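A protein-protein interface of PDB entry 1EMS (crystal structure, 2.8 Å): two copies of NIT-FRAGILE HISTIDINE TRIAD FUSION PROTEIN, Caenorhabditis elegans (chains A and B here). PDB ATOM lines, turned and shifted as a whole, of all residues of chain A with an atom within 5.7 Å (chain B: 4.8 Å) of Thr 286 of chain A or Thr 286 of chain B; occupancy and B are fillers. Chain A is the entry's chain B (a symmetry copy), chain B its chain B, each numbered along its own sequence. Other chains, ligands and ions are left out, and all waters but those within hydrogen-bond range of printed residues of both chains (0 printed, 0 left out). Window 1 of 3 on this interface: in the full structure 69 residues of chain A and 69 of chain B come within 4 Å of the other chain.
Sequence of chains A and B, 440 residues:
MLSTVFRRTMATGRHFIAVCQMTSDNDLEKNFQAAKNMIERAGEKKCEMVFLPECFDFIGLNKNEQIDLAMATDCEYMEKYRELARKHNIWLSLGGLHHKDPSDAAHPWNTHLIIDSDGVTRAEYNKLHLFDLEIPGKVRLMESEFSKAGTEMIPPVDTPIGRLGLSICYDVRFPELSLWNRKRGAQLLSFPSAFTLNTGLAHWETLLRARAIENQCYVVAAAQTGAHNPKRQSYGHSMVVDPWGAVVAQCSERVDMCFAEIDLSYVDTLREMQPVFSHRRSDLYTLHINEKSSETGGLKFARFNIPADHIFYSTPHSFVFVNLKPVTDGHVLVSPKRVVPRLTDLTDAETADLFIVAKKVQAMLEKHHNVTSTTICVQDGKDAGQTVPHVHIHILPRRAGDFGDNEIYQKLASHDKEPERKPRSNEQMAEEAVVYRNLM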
ATOM      1  N   ARG A 281     -12.870 -16.840   0.877  1.00  0.00           N
ATOM      2  CA  ARG A 281     -11.447 -16.541   0.944  1.00  0.00           C
ATOM      3  C   ARG A 281     -11.208 -15.170   0.342  1.00  0.00           C
ATOM      4  O   ARG A 281     -10.959 -15.044  -0.858  1.00  0.00           O
ATOM      5  CB  ARG A 281     -10.664 -17.602   0.179  1.00  0.00           C
ATOM      6  CG  ARG A 281     -10.994 -18.990   0.653  1.00  0.00           C
ATOM      7  CD  ARG A 281     -10.372 -19.287   1.996  1.00  0.00           C
ATOM      8  NE  ARG A 281      -9.157 -20.082   1.831  1.00  0.00           N
ATOM      9  CZ  ARG A 281      -7.950 -19.574   1.605  1.00  0.00           C
ATOM     10  NH1 ARG A 281      -7.781 -18.260   1.531  1.00  0.00           N
ATOM     11  NH2 ARG A 281      -6.916 -20.384   1.428  1.00  0.00           N
ATOM     12  N   SER A 282     -11.289 -14.140   1.180  1.00  0.00           N
ATOM     13  CA  SER A 282     -11.099 -12.773   0.711  1.00  0.00           C
ATOM     14  C   SER A 282      -9.645 -12.466   0.445  1.00  0.00           C
ATOM     15  O   SER A 282      -9.312 -11.443  -0.145  1.00  0.00           O
ATOM     16  CB  SER A 282     -11.660 -11.790   1.726  1.00  0.00           C
ATOM     17  OG  SER A 282     -13.071 -11.887   1.740  1.00  0.00           O
ATOM     18  N   LEU A 284      -7.920 -14.373  -1.365  1.00  0.00           N
ATOM     19  CA  LEU A 284      -7.676 -14.905  -2.693  1.00  0.00           C
ATOM     20  C   LEU A 284      -8.493 -14.201  -3.759  1.00  0.00           C
ATOM     21  O   LEU A 284      -8.020 -14.001  -4.871  1.00  0.00           O
ATOM     22  CB  LEU A 284      -7.963 -16.406  -2.713  1.00  0.00           C
ATOM     23  CG  LEU A 284      -7.106 -17.250  -1.765  1.00  0.00           C
ATOM     24  CD1 LEU A 284      -7.434 -18.733  -1.939  1.00  0.00           C
ATOM     25  CD2 LEU A 284      -5.636 -17.000  -2.051  1.00  0.00           C
ATOM     26  N   TYR A 285      -9.723 -13.827  -3.434  1.00  0.00           N
ATOM     27  CA  TYR A 285     -10.558 -13.135  -4.407  1.00  0.00           C
ATOM     28  C   TYR A 285     -11.386 -12.061  -3.730  1.00  0.00           C
ATOM     29  O   TYR A 285     -11.706 -12.168  -2.541  1.00  0.00           O
ATOM     30  CB  TYR A 285     -11.463 -14.128  -5.156  1.00  0.00           C
ATOM     31  CG  TYR A 285     -12.396 -14.960  -4.288  1.00  0.00           C
ATOM     32  CD1 TYR A 285     -13.538 -14.399  -3.709  1.00  0.00           C
ATOM     33  CD2 TYR A 285     -12.134 -16.314  -4.047  1.00  0.00           C
ATOM     34  CE1 TYR A 285     -14.393 -15.167  -2.912  1.00  0.00           C
ATOM     35  CE2 TYR A 285     -12.981 -17.091  -3.252  1.00  0.00           C
ATOM     36  CZ  TYR A 285     -14.106 -16.514  -2.687  1.00  0.00           C
ATOM     37  OH  TYR A 285     -14.939 -17.280  -1.896  1.00  0.00           O
ATOM     38  N   THR A 286     -11.725 -11.025  -4.494  1.00  0.00           N
ATOM     39  CA  THR A 286     -12.508  -9.904  -3.987  1.00  0.00           C
ATOM     40  C   THR A 286     -13.517  -9.423  -5.024  1.00  0.00           C
ATOM     41  O   THR A 286     -13.149  -9.113  -6.154  1.00  0.00           O
ATOM     42  CB  THR A 286     -11.578  -8.729  -3.628  1.00  0.00           C
ATOM     43  OG1 THR A 286     -10.731  -9.111  -2.538  1.00  0.00           O
ATOM     44  CG2 THR A 286     -12.376  -7.506  -3.246  1.00  0.00           C
ATOM     45  N   LEU A 287     -14.788  -9.359  -4.654  1.00  0.00           N
ATOM     46  CA  LEU A 287     -15.782  -8.887  -5.601  1.00  0.00           C
ATOM     47  C   LEU A 287     -15.955  -7.386  -5.445  1.00  0.00           C
ATOM     48  O   LEU A 287     -16.758  -6.932  -4.635  1.00  0.00           O
ATOM     49  CB  LEU A 287     -17.136  -9.573  -5.378  1.00  0.00           C
ATOM     50  CG  LEU A 287     -18.286  -8.953  -6.191  1.00  0.00           C
ATOM     51  CD1 LEU A 287     -18.007  -9.100  -7.679  1.00  0.00           C
ATOM     52  CD2 LEU A 287     -19.591  -9.612  -5.830  1.00  0.00           C
ATOM     53  N   HIS A 288     -15.208  -6.616  -6.222  1.00  0.00           N
ATOM     54  CA  HIS A 288     -15.304  -5.166  -6.147  1.00  0.00           C
ATOM     55  C   HIS A 288     -16.490  -4.595  -6.905  1.00  0.00           C
ATOM     56  O   HIS A 288     -16.754  -4.972  -8.048  1.00  0.00           O
ATOM     57  CB  HIS A 288     -14.044  -4.499  -6.693  1.00  0.00           C
ATOM     58  CG  HIS A 288     -14.180  -3.015  -6.816  1.00  0.00           C
ATOM     59  ND1 HIS A 288     -14.167  -2.178  -5.721  1.00  0.00           N
ATOM     60  CD2 HIS A 288     -14.449  -2.232  -7.887  1.00  0.00           C
ATOM     61  CE1 HIS A 288     -14.430  -0.944  -6.114  1.00  0.00           C
ATOM     62  NE2 HIS A 288     -14.606  -0.950  -7.423  1.00  0.00           N
ATOM     63  N   ILE A 289     -17.184  -3.659  -6.268  1.00  0.00           N
ATOM     64  CA  ILE A 289     -18.335  -3.002  -6.869  1.00  0.00           C
ATOM     65  C   ILE A 289     -18.158  -1.488  -6.785  1.00  0.00           C
ATOM     66  O   ILE A 289     -17.667  -0.963  -5.786  1.00  0.00           O
ATOM     67  CB  ILE A 289     -19.665  -3.386  -6.145  1.00  0.00           C
ATOM     68  CG1 ILE A 289     -20.132  -4.785  -6.567  1.00  0.00           C
ATOM     69  CG2 ILE A 289     -20.750  -2.360  -6.467  1.00  0.00           C
ATOM     70  CD1 ILE A 289     -19.218  -5.912  -6.134  1.00  0.00           C
ATOM     71  N   ASP A 348      -7.966  -6.212   0.384  1.00  0.00           N
ATOM     72  CA  ASP A 348      -8.078  -6.060  -1.057  1.00  0.00           C
ATOM     73  C   ASP A 348      -9.295  -5.255  -1.471  1.00  0.00           C
ATOM     74  O   ASP A 348      -9.233  -4.470  -2.414  1.00  0.00           O
ATOM     75  CB  ASP A 348      -8.108  -7.422  -1.743  1.00  0.00           C
ATOM     76  CG  ASP A 348      -6.830  -8.212  -1.534  1.00  0.00           C
ATOM     77  OD1 ASP A 348      -5.775  -7.601  -1.267  1.00  0.00           O
ATOM     78  OD2 ASP A 348      -6.874  -9.451  -1.656  1.00  0.00           O
ATOM     79  N   ALA A 349     -10.409  -5.438  -0.774  1.00  0.00           N
ATOM     80  CA  ALA A 349     -11.617  -4.701  -1.123  1.00  0.00           C
ATOM     81  C   ALA A 349     -11.316  -3.215  -1.037  1.00  0.00           C
ATOM     82  O   ALA A 349     -11.674  -2.440  -1.927  1.00  0.00           O
ATOM     83  CB  ALA A 349     -12.745  -5.067  -0.173  1.00  0.00           C
ATOM     84  N   ALA A 352      -8.315  -2.063  -3.595  1.00  0.00           N
ATOM     85  CA  ALA A 352      -8.937  -1.950  -4.909  1.00  0.00           C
ATOM     86  C   ALA A 352      -9.858  -0.736  -5.029  1.00  0.00           C
ATOM     87  O   ALA A 352      -9.746   0.044  -5.974  1.00  0.00           O
ATOM     88  CB  ALA A 352      -9.712  -3.222  -5.224  1.00  0.00           C
ATOM     89  N   ILE A 356      -9.333   2.706  -7.323  1.00  0.00           N
ATOM     90  CA  ILE A 356     -10.251   2.820  -8.450  1.00  0.00           C
ATOM     91  C   ILE A 356     -10.970   4.143  -8.254  1.00  0.00           C
ATOM     92  O   ILE A 356     -11.392   4.777  -9.217  1.00  0.00           O
ATOM     93  CB  ILE A 356     -11.292   1.674  -8.505  1.00  0.00           C
ATOM     94  CG1 ILE A 356     -10.608   0.374  -8.942  1.00  0.00           C
ATOM     95  CG2 ILE A 356     -12.428   2.048  -9.475  1.00  0.00           C
ATOM     96  CD1 ILE A 356     -11.535  -0.809  -9.022  1.00  0.00           C
ATOM     97  N   SER B 282     -18.438  -4.677 -16.375  1.00  0.00           N
ATOM     98  CA  SER B 282     -17.147  -4.558 -15.708  1.00  0.00           C
ATOM     99  C   SER B 282     -16.896  -3.153 -15.213  1.00  0.00           C
ATOM    100  O   SER B 282     -15.965  -2.907 -14.454  1.00  0.00           O
ATOM    101  CB  SER B 282     -16.032  -4.985 -16.648  1.00  0.00           C
ATOM    102  OG  SER B 282     -16.108  -6.381 -16.861  1.00  0.00           O
ATOM    103  N   LEU B 284     -19.047  -1.674 -13.460  1.00  0.00           N
ATOM    104  CA  LEU B 284     -19.753  -1.606 -12.194  1.00  0.00           C
ATOM    105  C   LEU B 284     -19.185  -2.560 -11.161  1.00  0.00           C
ATOM    106  O   LEU B 284     -19.141  -2.241  -9.980  1.00  0.00           O
ATOM    107  CB  LEU B 284     -21.240  -1.885 -12.411  1.00  0.00           C
ATOM    108  CG  LEU B 284     -21.962  -0.906 -13.341  1.00  0.00           C
ATOM    109  CD1 LEU B 284     -23.450  -1.245 -13.410  1.00  0.00           C
ATOM    110  CD2 LEU B 284     -21.770   0.513 -12.833  1.00  0.00           C
ATOM    111  N   TYR B 285     -18.756  -3.738 -11.594  1.00  0.00           N
ATOM    112  CA  TYR B 285     -18.189  -4.699 -10.656  1.00  0.00           C
ATOM    113  C   TYR B 285     -17.024  -5.435 -11.288  1.00  0.00           C
ATOM    114  O   TYR B 285     -16.970  -5.594 -12.513  1.00  0.00           O
ATOM    115  CB  TYR B 285     -19.261  -5.690 -10.171  1.00  0.00           C
ATOM    116  CG  TYR B 285     -19.959  -6.495 -11.258  1.00  0.00           C
ATOM    117  CD1 TYR B 285     -19.312  -7.553 -11.903  1.00  0.00           C
ATOM    118  CD2 TYR B 285     -21.272  -6.197 -11.639  1.00  0.00           C
ATOM    119  CE1 TYR B 285     -19.957  -8.291 -12.901  1.00  0.00           C
ATOM    120  CE2 TYR B 285     -21.927  -6.926 -12.636  1.00  0.00           C
ATOM    121  CZ  TYR B 285     -21.267  -7.969 -13.263  1.00  0.00           C
ATOM    122  OH  TYR B 285     -21.911  -8.686 -14.252  1.00  0.00           O
ATOM    123  N   THR B 286     -16.095  -5.878 -10.445  1.00  0.00           N
ATOM    124  CA  THR B 286     -14.906  -6.592 -10.898  1.00  0.00           C
ATOM    125  C   THR B 286     -14.555  -7.732  -9.949  1.00  0.00           C
ATOM    126  O   THR B 286     -14.402  -7.519  -8.749  1.00  0.00           O
ATOM    127  CB  THR B 286     -13.707  -5.629 -10.971  1.00  0.00           C
ATOM    128  OG1 THR B 286     -13.951  -4.643 -11.981  1.00  0.00           O
ATOM    129  CG2 THR B 286     -12.434  -6.375 -11.290  1.00  0.00           C
ATOM    130  N   LEU B 287     -14.426  -8.943 -10.472  1.00  0.00           N
ATOM    131  CA  LEU B 287     -14.071 -10.057  -9.611  1.00  0.00           C
ATOM    132  C   LEU B 287     -12.560 -10.216  -9.588  1.00  0.00           C
ATOM    133  O   LEU B 287     -11.993 -10.907 -10.429  1.00  0.00           O
ATOM    134  CB  LEU B 287     -14.705 -11.366 -10.099  1.00  0.00           C
ATOM    135  CG  LEU B 287     -14.183 -12.617  -9.371  1.00  0.00           C
ATOM    136  CD1 LEU B 287     -14.529 -12.537  -7.891  1.00  0.00           C
ATOM    137  CD2 LEU B 287     -14.772 -13.859  -9.985  1.00  0.00           C
ATOM    138  N   HIS B 288     -11.910  -9.582  -8.623  1.00  0.00           N
ATOM    139  CA  HIS B 288     -10.462  -9.675  -8.517  1.00  0.00           C
ATOM    140  C   HIS B 288      -9.981 -10.954  -7.853  1.00  0.00           C
ATOM    141  O   HIS B 288     -10.502 -11.366  -6.815  1.00  0.00           O
ATOM    142  CB  HIS B 288      -9.888  -8.502  -7.726  1.00  0.00           C
ATOM    143  CG  HIS B 288      -8.432  -8.660  -7.426  1.00  0.00           C
ATOM    144  ND1 HIS B 288      -7.458  -8.507  -8.389  1.00  0.00           N
ATOM    145  CD2 HIS B 288      -7.794  -9.074  -6.305  1.00  0.00           C
ATOM    146  CE1 HIS B 288      -6.283  -8.826  -7.874  1.00  0.00           C
ATOM    147  NE2 HIS B 288      -6.460  -9.174  -6.612  1.00  0.00           N
ATOM    148  N   ASP B 348     -10.727  -1.530 -14.101  1.00  0.00           N
ATOM    149  CA  ASP B 348     -10.765  -1.833 -12.681  1.00  0.00           C
ATOM    150  C   ASP B 348     -10.007  -3.099 -12.328  1.00  0.00           C
ATOM    151  O   ASP B 348      -9.354  -3.166 -11.290  1.00  0.00           O
ATOM    152  CB  ASP B 348     -12.205  -1.947 -12.191  1.00  0.00           C
ATOM    153  CG  ASP B 348     -12.977  -0.648 -12.333  1.00  0.00           C
ATOM    154  OD1 ASP B 348     -12.349   0.429 -12.374  1.00  0.00           O
ATOM    155  OD2 ASP B 348     -14.220  -0.701 -12.383  1.00  0.00           O
ATOM    156  N   ALA B 349     -10.082  -4.109 -13.184  1.00  0.00           N
ATOM    157  CA  ALA B 349      -9.383  -5.357 -12.903  1.00  0.00           C
ATOM    158  C   ALA B 349      -7.902  -5.054 -12.750  1.00  0.00           C
ATOM    159  O   ALA B 349      -7.247  -5.531 -11.821  1.00  0.00           O
ATOM    160  CB  ALA B 349      -9.605  -6.347 -14.034  1.00  0.00           C
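N of Arg 281 of chain A is in hydrogen-bond range of OH of Tyr 285 of chain A, 3.5 Å away.
Among the printed residues, merely in contact across the chains: Tyr 285 of chain A with His 288 of chain B, His 288 of chain A with Tyr 285 of chain B, Ile 289 of chain A with Leu 284 of chain B, Ile 356 of chain A with Asp 348 of chain B, Leu 287 of chain A with Thr 286 of chain B, Thr 286 of chain A with Leu 287 of chain B and Ile 289 of chain A with Tyr 285 of chain B.
Tyr 285 of chain A touches His 288 of chain B, and with the chains exchanged His 288 of chain A touches Tyr 285 of chain B. Thr 286 of chain A touches its own counterpart, Thr 286 of chain B. Thr 286 of chain A touches Leu 287 of chain B, and with the chains exchanged Leu 287 of chain A touches Thr 286 of chain B. Thr 286 of chain A touches His 288 of chain B, and with the chains exchanged His 288 of chain A touches Thr 286 of chain B. Of the 10 pairs that touch across the chains among the printed residues, 7 have their exchanged pair printed and touching as well.
The backbone carbonyl oxygen (O) of His 288 of chain A sits at hydrogen-bond distance from the backbone NH (N) of Thr 286 of chain B. O of Thr 286 of chain B lies close to O of Thr 286 of chain A (3.3 Å). The backbone NH of Thr 286 of chain A lies within hydrogen-bond range of the backbone carbonyl oxygen of His 288 of chain B, at 2.6 Å.
Thr 286 of chain A touches just these residues of chain B: Thr 286 (3.3 Å), Leu 287 (3.7 Å) and His 288 (2.6 Å). Thr 286 of chain B touches just these residues of chain A: Thr 286, Leu 287 and His 288. Printed residues of chain A within 4 Å of Leu 284 of chain B: Ile 289. Of the printed residues of chain B, Ile 289 of chain A touches Leu 284 (3.3 Å) and Tyr 285 (3.8 Å). Of the printed residues of chain B, Tyr 285 of chain A touches His 288 (3.0 Å). Ala 349 of chain A touches none of the printed residues of chain B.
Of the 12 printed residues of chain A, 6 touch a printed residue of chain B. Printed residues of chain A that touch a printed residue of chain B: Tyr 285, Thr 286, Leu 287, His 288, Ile 289 and Ile 356. Hydrophobic or aromatic side chains of chain A within 4 Å of the printed part of chain B: Tyr 285, His 288, Ile 289 and Ile 356. Of the 8 printed residues of chain B, 6 touch a printed residue of chain A. Printed residues of chain B that touch a printed residue of chain A: Leu 284, Tyr 285, Thr 286, Leu 287, His 288 and Asp 348. Hydrophobic or aromatic side chains of chain B within 4 Å of the printed part of chain A: Tyr 285 and His 288. Along chain B the printed residues that touch a printed residue of chain A span positions 284 to 348. Among the printed residues, 10 pairs touch across the chains. Among the printed residues, no Asp or Glu carboxylate lies within 4 Å of a Lys or Arg side-chain nitrogen of the other chain.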
